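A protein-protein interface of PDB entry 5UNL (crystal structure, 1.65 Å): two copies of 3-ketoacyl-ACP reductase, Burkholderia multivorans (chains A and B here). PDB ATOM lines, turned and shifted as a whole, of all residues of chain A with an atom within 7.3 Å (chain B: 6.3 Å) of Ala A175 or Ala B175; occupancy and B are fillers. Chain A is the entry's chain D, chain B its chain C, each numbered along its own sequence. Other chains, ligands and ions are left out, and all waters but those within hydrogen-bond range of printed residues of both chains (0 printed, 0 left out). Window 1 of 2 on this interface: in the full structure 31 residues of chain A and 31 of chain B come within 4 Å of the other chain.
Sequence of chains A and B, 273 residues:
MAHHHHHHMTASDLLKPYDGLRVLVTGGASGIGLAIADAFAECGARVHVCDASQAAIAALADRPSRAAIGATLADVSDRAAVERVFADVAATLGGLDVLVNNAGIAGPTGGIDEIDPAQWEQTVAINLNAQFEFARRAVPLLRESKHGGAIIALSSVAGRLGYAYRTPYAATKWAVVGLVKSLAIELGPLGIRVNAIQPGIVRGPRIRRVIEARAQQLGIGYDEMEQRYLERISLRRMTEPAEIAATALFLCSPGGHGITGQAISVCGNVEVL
O of Gly A178 is in hydrogen-bond range of OG of Ser A182, at 2.7 Å. The backbone carbonyl oxygen (O) of Ala A158 lies close to the indole nitrogen (NE1) of Trp A174, 3.0 Å away.
Ala A175 touches just these residues of chain B: Ala B171 and Ala B175. Ala B175 touches two residues of chain A. Printed residues of chain B within 4 Å of Thr A167: Leu B179 (3.7 Å). Of the printed residues of chain A, Ala B170 touches Ser A182. The nearest residue of chain B that does not touch Ala A175 is Trp B174 (4.2 Å). The nearest residue of chain A that does not touch Ala B175 is Trp A174 (4.3 Å). The nearest printed residue of chain A that does not touch Val B177 is Ala A171 (6.7 Å).
Ala A171 touches Ala B175, and with the chains exchanged Ala A175 touches Ala B171. Trp B174 touches its own counterpart, Trp A174. Trp A174 touches Val B177, and with the chains exchanged Val A177 touches Trp B174. Trp A174 touches Gly B178, and with the chains exchanged Gly A178 touches Trp B174.
Printed residues of chain A that touch a printed residue of chain B: Thr A167, Ala A171, Trp A174, Ala A175, Val A177, Gly A178, Lys A181 and Ser A182. Of the 13 printed residues of chain B, 7 touch a printed residue of chain A. Hydrophobic or aromatic side chains of chain B within 4 Å of the printed part of chain A: Ala B170, Ala B171, Trp B174, Ala B175, Val B177 and Leu B179. Among the printed residues, no Asp or Glu carboxylate lies within 4 Å of a Lys or Arg side-chain nitrogen of the other chain.
CD1 of Leu B179 touches CB of Thr A167 (3.7 Å). Trp B174 touches Trp A174. Val B177 touches Trp A174 (CG1 to CZ3, 3.6 Å). Trp A174 touches Gly B178 (CG to CA, 3.4 Å). CB of Ala A175 touches O of Ala B171 (3.3 Å). Ala A175 touches Ala B175 (CB to CB, 3.9 Å). CZ3 of Trp B174 touches CG1 of Val A177, 3.5 Å away. Gly A178 touches Trp B174 (CA to CG, 3.4 Å). Lys A181 touches Trp B174 (CE to CH2, 3.9 Å). OG of Ser A182 touches CB of Ala B170, at 3.2 Å.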
ATOM      1  N   TRP A 120       6.138  10.533  -7.787  1.00  0.00           N
ATOM      2  CA  TRP A 120       6.565  11.898  -8.099  1.00  0.00           C
ATOM      3  C   TRP A 120       8.085  11.980  -8.200  1.00  0.00           C
ATOM      4  O   TRP A 120       8.631  12.488  -9.185  1.00  0.00           O
ATOM      5  CB  TRP A 120       6.057  12.888  -7.033  1.00  0.00           C
ATOM      6  CG  TRP A 120       6.670  14.265  -7.184  1.00  0.00           C
ATOM      7  CD1 TRP A 120       7.943  14.639  -6.826  1.00  0.00           C
ATOM      8  CD2 TRP A 120       6.064  15.436  -7.771  1.00  0.00           C
ATOM      9  NE1 TRP A 120       8.156  15.961  -7.149  1.00  0.00           N
ATOM     10  CE2 TRP A 120       7.019  16.474  -7.713  1.00  0.00           C
ATOM     11  CE3 TRP A 120       4.804  15.710  -8.314  1.00  0.00           C
ATOM     12  CZ2 TRP A 120       6.762  17.757  -8.198  1.00  0.00           C
ATOM     13  CZ3 TRP A 120       4.548  16.995  -8.792  1.00  0.00           C
ATOM     14  CH2 TRP A 120       5.522  17.999  -8.729  1.00  0.00           C
ATOM     15  N   ASN A 127      13.064  12.155 -15.575  1.00  0.00           N
ATOM     16  CA  ASN A 127      12.770  13.156 -16.594  1.00  0.00           C
ATOM     17  C   ASN A 127      13.646  14.390 -16.485  1.00  0.00           C
ATOM     18  O   ASN A 127      13.871  15.059 -17.497  1.00  0.00           O
ATOM     19  CB  ASN A 127      11.309  13.588 -16.515  1.00  0.00           C
ATOM     20  CG  ASN A 127      10.375  12.512 -16.988  1.00  0.00           C
ATOM     21  OD1 ASN A 127      10.808  11.393 -17.284  1.00  0.00           O
ATOM     22  ND2 ASN A 127       9.080  12.830 -17.052  1.00  0.00           N
ATOM     23  N   LEU A 128      14.121  14.718 -15.284  1.00  0.00           N
ATOM     24  CA  LEU A 128      14.926  15.919 -15.080  1.00  0.00           C
ATOM     25  C   LEU A 128      16.338  15.594 -14.616  1.00  0.00           C
ATOM     26  O   LEU A 128      17.307  16.001 -15.271  1.00  0.00           O
ATOM     27  CB  LEU A 128      14.243  16.863 -14.080  1.00  0.00           C
ATOM     28  CG  LEU A 128      15.088  18.100 -13.732  1.00  0.00           C
ATOM     29  CD1 LEU A 128      15.365  18.924 -14.988  1.00  0.00           C
ATOM     30  CD2 LEU A 128      14.368  18.944 -12.683  1.00  0.00           C
ATOM     31  N   SER A 155      11.397  17.366 -24.469  1.00  0.00           N
ATOM     32  CA  SER A 155      10.358  17.886 -23.594  1.00  0.00           C
ATOM     33  C   SER A 155       9.028  17.289 -24.056  1.00  0.00           C
ATOM     34  O   SER A 155       8.979  16.125 -24.472  1.00  0.00           O
ATOM     35  CB  SER A 155      10.354  19.422 -23.638  1.00  0.00           C
ATOM     36  OG  SER A 155       9.369  19.993 -22.779  1.00  0.00           O
ATOM     37  N   ALA A 158       3.449  19.201 -22.879  1.00  0.00           N
ATOM     38  CA  ALA A 158       3.231  19.501 -21.463  1.00  0.00           C
ATOM     39  C   ALA A 158       4.344  20.343 -20.856  1.00  0.00           C
ATOM     40  O   ALA A 158       4.271  20.673 -19.668  1.00  0.00           O
ATOM     41  CB  ALA A 158       3.074  18.196 -20.671  1.00  0.00           C
ATOM     42  N   GLY A 159       5.366  20.682 -21.628  1.00  0.00           N
ATOM     43  CA  GLY A 159       6.374  21.645 -21.220  1.00  0.00           C
ATOM     44  C   GLY A 159       6.077  23.065 -21.636  1.00  0.00           C
ATOM     45  O   GLY A 159       6.856  23.969 -21.313  1.00  0.00           O
ATOM     46  N   THR A 167       0.832  16.511 -12.859  1.00  0.00           N
ATOM     47  CA  THR A 167       1.723  17.562 -12.376  1.00  0.00           C
ATOM     48  C   THR A 167       3.206  17.183 -12.369  1.00  0.00           C
ATOM     49  O   THR A 167       4.020  18.033 -12.764  1.00  0.00           O
ATOM     50  CB  THR A 167       1.284  18.049 -10.982  1.00  0.00           C
ATOM     51  OG1 THR A 167       1.093  16.945 -10.083  1.00  0.00           O
ATOM     52  CG2 THR A 167       0.016  18.893 -11.064  1.00  0.00           C
ATOM     53  N   TYR A 169       4.824  15.139 -14.366  1.00  0.00           N
ATOM     54  CA  TYR A 169       5.210  15.139 -15.768  1.00  0.00           C
ATOM     55  C   TYR A 169       5.357  16.562 -16.297  1.00  0.00           C
ATOM     56  O   TYR A 169       6.397  16.918 -16.867  1.00  0.00           O
ATOM     57  CB  TYR A 169       4.180  14.362 -16.580  1.00  0.00           C
ATOM     58  CG  TYR A 169       4.553  14.193 -18.033  1.00  0.00           C
ATOM     59  CD1 TYR A 169       5.482  13.241 -18.418  1.00  0.00           C
ATOM     60  CD2 TYR A 169       3.955  14.975 -19.023  1.00  0.00           C
ATOM     61  CE1 TYR A 169       5.815  13.061 -19.762  1.00  0.00           C
ATOM     62  CE2 TYR A 169       4.276  14.802 -20.354  1.00  0.00           C
ATOM     63  CZ  TYR A 169       5.204  13.856 -20.717  1.00  0.00           C
ATOM     64  OH  TYR A 169       5.521  13.702 -22.048  1.00  0.00           O
ATOM     65  N   ALA A 170       4.341  17.401 -16.083  1.00  0.00           N
ATOM     66  CA  ALA A 170       4.400  18.773 -16.583  1.00  0.00           C
ATOM     67  C   ALA A 170       5.556  19.538 -15.947  1.00  0.00           C
ATOM     68  O   ALA A 170       6.321  20.210 -16.646  1.00  0.00           O
ATOM     69  CB  ALA A 170       3.074  19.494 -16.343  1.00  0.00           C
ATOM     70  N   ALA A 171       5.703  19.442 -14.616  1.00  0.00           N
ATOM     71  CA  ALA A 171       6.827  20.094 -13.948  1.00  0.00           C
ATOM     72  C   ALA A 171       8.154  19.746 -14.618  1.00  0.00           C
ATOM     73  O   ALA A 171       8.969  20.631 -14.894  1.00  0.00           O
ATOM     74  CB  ALA A 171       6.879  19.708 -12.471  1.00  0.00           C
ATOM     75  N   THR A 172       8.390  18.462 -14.888  1.00  0.00           N
ATOM     76  CA  THR A 172       9.688  18.096 -15.466  1.00  0.00           C
ATOM     77  C   THR A 172       9.820  18.563 -16.902  1.00  0.00           C
ATOM     78  O   THR A 172      10.928  18.894 -17.340  1.00  0.00           O
ATOM     79  CB  THR A 172       9.946  16.590 -15.410  1.00  0.00           C
ATOM     80  OG1 THR A 172       8.962  15.873 -16.177  1.00  0.00           O
ATOM     81  CG2 THR A 172       9.971  16.094 -13.966  1.00  0.00           C
ATOM     82  N   LYS A 173       8.723  18.599 -17.654  1.00  0.00           N
ATOM     83  CA  LYS A 173       8.862  18.995 -19.050  1.00  0.00           C
ATOM     84  C   LYS A 173       9.074  20.496 -19.172  1.00  0.00           C
ATOM     85  O   LYS A 173       9.788  20.940 -20.079  1.00  0.00           O
ATOM     86  CB  LYS A 173       7.656  18.514 -19.855  1.00  0.00           C
ATOM     87  CG  LYS A 173       7.548  16.978 -19.878  1.00  0.00           C
ATOM     88  CD  LYS A 173       8.779  16.351 -20.529  1.00  0.00           C
ATOM     89  CE  LYS A 173       8.778  14.833 -20.440  1.00  0.00           C
ATOM     90  NZ  LYS A 173       9.995  14.242 -21.028  1.00  0.00           N
ATOM     91  N   TRP A 174       8.503  21.281 -18.250  1.00  0.00           N
ATOM     92  CA  TRP A 174       8.842  22.701 -18.149  1.00  0.00           C
ATOM     93  C   TRP A 174      10.276  22.886 -17.672  1.00  0.00           C
ATOM     94  O   TRP A 174      10.985  23.774 -18.153  1.00  0.00           O
ATOM     95  CB  TRP A 174       7.876  23.414 -17.195  1.00  0.00           C
ATOM     96  CG  TRP A 174       6.542  23.732 -17.819  1.00  0.00           C
ATOM     97  CD1 TRP A 174       5.535  22.852 -18.075  1.00  0.00           C
ATOM     98  CD2 TRP A 174       6.064  25.021 -18.242  1.00  0.00           C
ATOM     99  NE1 TRP A 174       4.463  23.505 -18.631  1.00  0.00           N
ATOM    100  CE2 TRP A 174       4.765  24.835 -18.756  1.00  0.00           C
ATOM    101  CE3 TRP A 174       6.602  26.308 -18.231  1.00  0.00           C
ATOM    102  CZ2 TRP A 174       4.000  25.888 -19.265  1.00  0.00           C
ATOM    103  CZ3 TRP A 174       5.855  27.349 -18.767  1.00  0.00           C
ATOM    104  CH2 TRP A 174       4.561  27.135 -19.260  1.00  0.00           C
ATOM    105  N   ALA A 175      10.723  22.045 -16.734  1.00  0.00           N
ATOM    106  CA  ALA A 175      12.097  22.147 -16.261  1.00  0.00           C
ATOM    107  C   ALA A 175      13.084  21.936 -17.400  1.00  0.00           C
ATOM    108  O   ALA A 175      14.109  22.630 -17.479  1.00  0.00           O
ATOM    109  CB  ALA A 175      12.357  21.117 -15.159  1.00  0.00           C
ATOM    110  N   VAL A 176      12.799  20.968 -18.281  1.00  0.00           N
ATOM    111  CA  VAL A 176      13.682  20.698 -19.414  1.00  0.00           C
ATOM    112  C   VAL A 176      13.823  21.940 -20.292  1.00  0.00           C
ATOM    113  O   VAL A 176      14.924  22.262 -20.765  1.00  0.00           O
ATOM    114  CB  VAL A 176      13.181  19.480 -20.220  1.00  0.00           C
ATOM    115  CG1 VAL A 176      13.923  19.366 -21.579  1.00  0.00           C
ATOM    116  CG2 VAL A 176      13.365  18.194 -19.412  1.00  0.00           C
ATOM    117  N   VAL A 177      12.726  22.668 -20.507  1.00  0.00           N
ATOM    118  CA  VAL A 177      12.802  23.894 -21.301  1.00  0.00           C
ATOM    119  C   VAL A 177      13.761  24.894 -20.653  1.00  0.00           C
ATOM    120  O   VAL A 177      14.652  25.450 -21.314  1.00  0.00           O
ATOM    121  CB  VAL A 177      11.404  24.501 -21.507  1.00  0.00           C
ATOM    122  CG1 VAL A 177      11.517  25.829 -22.249  1.00  0.00           C
ATOM    123  CG2 VAL A 177      10.518  23.542 -22.300  1.00  0.00           C
ATOM    124  N   GLY A 178      13.608  25.130 -19.347  1.00  0.00           N
ATOM    125  CA  GLY A 178      14.517  26.052 -18.674  1.00  0.00           C
ATOM    126  C   GLY A 178      15.949  25.560 -18.671  1.00  0.00           C
ATOM    127  O   GLY A 178      16.892  26.358 -18.755  1.00  0.00           O
ATOM    128  N   LEU A 179      16.137  24.244 -18.572  1.00  0.00           N
ATOM    129  CA  LEU A 179      17.481  23.691 -18.616  1.00  0.00           C
ATOM    130  C   LEU A 179      18.104  23.918 -19.987  1.00  0.00           C
ATOM    131  O   LEU A 179      19.263  24.331 -20.089  1.00  0.00           O
ATOM    132  CB  LEU A 179      17.422  22.204 -18.246  1.00  0.00           C
ATOM    133  CG  LEU A 179      18.721  21.413 -18.406  1.00  0.00           C
ATOM    134  CD1 LEU A 179      19.791  21.981 -17.488  1.00  0.00           C
ATOM    135  CD2 LEU A 179      18.456  19.934 -18.081  1.00  0.00           C
ATOM    136  N   VAL A 180      17.313  23.723 -21.047  1.00  0.00           N
ATOM    137  CA  VAL A 180      17.780  23.975 -22.408  1.00  0.00           C
ATOM    138  C   VAL A 180      18.151  25.442 -22.586  1.00  0.00           C
ATOM    139  O   VAL A 180      19.216  25.772 -23.124  1.00  0.00           O
ATOM    140  CB  VAL A 180      16.709  23.533 -23.426  1.00  0.00           C
ATOM    141  CG1 VAL A 180      16.868  24.250 -24.758  1.00  0.00           C
ATOM    142  CG2 VAL A 180      16.743  22.012 -23.599  1.00  0.00           C
ATOM    143  N   LYS A 181      17.289  26.353 -22.128  1.00  0.00           N
ATOM    144  CA  LYS A 181      17.587  27.756 -22.380  1.00  0.00           C
ATOM    145  C   LYS A 181      18.805  28.205 -21.590  1.00  0.00           C
ATOM    146  O   LYS A 181      19.585  29.032 -22.072  1.00  0.00           O
ATOM    147  CB  LYS A 181      16.367  28.621 -22.067  1.00  0.00           C
ATOM    148  CG  LYS A 181      15.258  28.401 -23.091  1.00  0.00           C
ATOM    149  CD  LYS A 181      14.215  29.493 -23.022  1.00  0.00           C
ATOM    150  CE  LYS A 181      12.980  29.098 -23.809  1.00  0.00           C
ATOM    151  NZ  LYS A 181      13.156  29.207 -25.283  1.00  0.00           N
ATOM    152  N   SER A 182      19.014  27.641 -20.401  1.00  0.00           N
ATOM    153  CA  SER A 182      20.215  27.970 -19.639  1.00  0.00           C
ATOM    154  C   SER A 182      21.465  27.387 -20.290  1.00  0.00           C
ATOM    155  O   SER A 182      22.485  28.076 -20.416  1.00  0.00           O
ATOM    156  CB  SER A 182      20.076  27.457 -18.207  1.00  0.00           C
ATOM    157  OG  SER A 182      18.864  27.897 -17.640  1.00  0.00           O
ATOM    158  N   LEU B 128      11.733  22.108  -5.902  1.00  0.00           N
ATOM    159  CA  LEU B 128      10.671  21.466  -6.664  1.00  0.00           C
ATOM    160  C   LEU B 128       9.956  20.416  -5.834  1.00  0.00           C
ATOM    161  O   LEU B 128       8.742  20.531  -5.618  1.00  0.00           O
ATOM    162  CB  LEU B 128      11.239  20.847  -7.953  1.00  0.00           C
ATOM    163  CG  LEU B 128      10.216  20.069  -8.794  1.00  0.00           C
ATOM    164  CD1 LEU B 128       9.043  20.951  -9.169  1.00  0.00           C
ATOM    165  CD2 LEU B 128      10.892  19.518 -10.045  1.00  0.00           C
ATOM    166  N   GLY B 159      12.882  31.497 -13.893  1.00  0.00           N
ATOM    167  CA  GLY B 159      11.882  30.586 -14.408  1.00  0.00           C
ATOM    168  C   GLY B 159      11.223  31.040 -15.687  1.00  0.00           C
ATOM    169  O   GLY B 159      10.350  30.335 -16.197  1.00  0.00           O
ATOM    170  N   ALA B 170      17.632  27.350 -12.445  1.00  0.00           N
ATOM    171  CA  ALA B 170      16.717  27.686 -13.534  1.00  0.00           C
ATOM    172  C   ALA B 170      15.754  26.536 -13.805  1.00  0.00           C
ATOM    173  O   ALA B 170      14.541  26.742 -13.926  1.00  0.00           O
ATOM    174  CB  ALA B 170      17.501  28.051 -14.793  1.00  0.00           C
ATOM    175  N   ALA B 171      16.272  25.306 -13.874  1.00  0.00           N
ATOM    176  CA  ALA B 171      15.388  24.172 -14.147  1.00  0.00           C
ATOM    177  C   ALA B 171      14.264  24.096 -13.123  1.00  0.00           C
ATOM    178  O   ALA B 171      13.096  23.885 -13.479  1.00  0.00           O
ATOM    179  CB  ALA B 171      16.181  22.865 -14.180  1.00  0.00           C
ATOM    180  N   THR B 172      14.589  24.259 -11.836  1.00  0.00           N
ATOM    181  CA  THR B 172      13.535  24.160 -10.833  1.00  0.00           C
ATOM    182  C   THR B 172      12.573  25.333 -10.909  1.00  0.00           C
ATOM    183  O   THR B 172      11.379  25.162 -10.644  1.00  0.00           O
ATOM    184  CB  THR B 172      14.105  24.061  -9.416  1.00  0.00           C
ATOM    185  OG1 THR B 172      14.888  25.225  -9.102  1.00  0.00           O
ATOM    186  CG2 THR B 172      14.954  22.812  -9.246  1.00  0.00           C
ATOM    187  N   LYS B 173      13.057  26.521 -11.263  1.00  0.00           N
ATOM    188  CA  LYS B 173      12.151  27.659 -11.289  1.00  0.00           C
ATOM    189  C   LYS B 173      11.230  27.625 -12.508  1.00  0.00           C
ATOM    190  O   LYS B 173      10.089  28.080 -12.418  1.00  0.00           O
ATOM    191  CB  LYS B 173      12.949  28.967 -11.205  1.00  0.00           C
ATOM    192  CG  LYS B 173      13.710  29.135  -9.874  1.00  0.00           C
ATOM    193  CD  LYS B 173      12.727  29.092  -8.687  1.00  0.00           C
ATOM    194  CE  LYS B 173      13.431  29.308  -7.341  1.00  0.00           C
ATOM    195  NZ  LYS B 173      12.509  29.174  -6.180  1.00  0.00           N
ATOM    196  N   TRP B 174      11.681  27.056 -13.632  1.00  0.00           N
ATOM    197  CA  TRP B 174      10.774  26.759 -14.736  1.00  0.00           C
ATOM    198  C   TRP B 174       9.785  25.672 -14.338  1.00  0.00           C
ATOM    199  O   TRP B 174       8.611  25.726 -14.718  1.00  0.00           O
ATOM    200  CB  TRP B 174      11.569  26.314 -15.975  1.00  0.00           C
ATOM    201  CG  TRP B 174      12.160  27.454 -16.745  1.00  0.00           C
ATOM    202  CD1 TRP B 174      13.226  28.221 -16.387  1.00  0.00           C
ATOM    203  CD2 TRP B 174      11.697  27.972 -17.997  1.00  0.00           C
ATOM    204  NE1 TRP B 174      13.456  29.182 -17.333  1.00  0.00           N
ATOM    205  CE2 TRP B 174      12.535  29.051 -18.338  1.00  0.00           C
ATOM    206  CE3 TRP B 174      10.651  27.627 -18.866  1.00  0.00           C
ATOM    207  CZ2 TRP B 174      12.355  29.796 -19.499  1.00  0.00           C
ATOM    208  CZ3 TRP B 174      10.481  28.375 -20.026  1.00  0.00           C
ATOM    209  CH2 TRP B 174      11.343  29.433 -20.336  1.00  0.00           C
ATOM    210  N   ALA B 175      10.247  24.668 -13.579  1.00  0.00           N
ATOM    211  CA  ALA B 175       9.350  23.602 -13.140  1.00  0.00           C
ATOM    212  C   ALA B 175       8.192  24.149 -12.313  1.00  0.00           C
ATOM    213  O   ALA B 175       7.051  23.675 -12.437  1.00  0.00           O
ATOM    214  CB  ALA B 175      10.128  22.559 -12.331  1.00  0.00           C
ATOM    215  N   VAL B 176       8.469  25.135 -11.455  1.00  0.00           N
ATOM    216  CA  VAL B 176       7.417  25.699 -10.611  1.00  0.00           C
ATOM    217  C   VAL B 176       6.331  26.337 -11.470  1.00  0.00           C
ATOM    218  O   VAL B 176       5.139  26.235 -11.156  1.00  0.00           O
ATOM    219  CB  VAL B 176       8.020  26.698  -9.607  1.00  0.00           C
ATOM    220  CG1 VAL B 176       6.917  27.545  -8.960  1.00  0.00           C
ATOM    221  CG2 VAL B 176       8.846  25.950  -8.544  1.00  0.00           C
ATOM    222  N   VAL B 177       6.717  27.000 -12.566  1.00  0.00           N
ATOM    223  CA  VAL B 177       5.727  27.560 -13.487  1.00  0.00           C
ATOM    224  C   VAL B 177       4.838  26.455 -14.057  1.00  0.00           C
ATOM    225  O   VAL B 177       3.607  26.567 -14.062  1.00  0.00           O
ATOM    226  CB  VAL B 177       6.413  28.357 -14.608  1.00  0.00           C
ATOM    227  CG1 VAL B 177       5.353  28.880 -15.597  1.00  0.00           C
ATOM    228  CG2 VAL B 177       7.246  29.525 -14.022  1.00  0.00           C
ATOM    229  N   GLY B 178       5.442  25.377 -14.566  1.00  0.00           N
ATOM    230  CA  GLY B 178       4.624  24.297 -15.110  1.00  0.00           C
ATOM    231  C   GLY B 178       3.736  23.661 -14.055  1.00  0.00           C
ATOM    232  O   GLY B 178       2.586  23.292 -14.326  1.00  0.00           O
ATOM    233  N   LEU B 179       4.254  23.535 -12.830  1.00  0.00           N
ATOM    234  CA  LEU B 179       3.450  22.994 -11.743  1.00  0.00           C
ATOM    235  C   LEU B 179       2.267  23.901 -11.452  1.00  0.00           C
ATOM    236  O   LEU B 179       1.139  23.425 -11.268  1.00  0.00           O
ATOM    237  CB  LEU B 179       4.322  22.813 -10.500  1.00  0.00           C
ATOM    238  CG  LEU B 179       3.648  22.334  -9.218  1.00  0.00           C
ATOM    239  CD1 LEU B 179       2.915  21.000  -9.437  1.00  0.00           C
ATOM    240  CD2 LEU B 179       4.671  22.191  -8.112  1.00  0.00           C
ATOM    241  N   VAL B 180       2.509  25.213 -11.433  1.00  0.00           N
ATOM    242  CA  VAL B 180       1.450  26.189 -11.188  1.00  0.00           C
ATOM    243  C   VAL B 180       0.390  26.116 -12.279  1.00  0.00           C
ATOM    244  O   VAL B 180      -0.808  26.087 -11.994  1.00  0.00           O
ATOM    245  CB  VAL B 180       2.050  27.602 -11.088  1.00  0.00           C
ATOM    246  CG1 VAL B 180       1.001  28.660 -11.406  1.00  0.00           C
ATOM    247  CG2 VAL B 180       2.641  27.821  -9.718  1.00  0.00           C
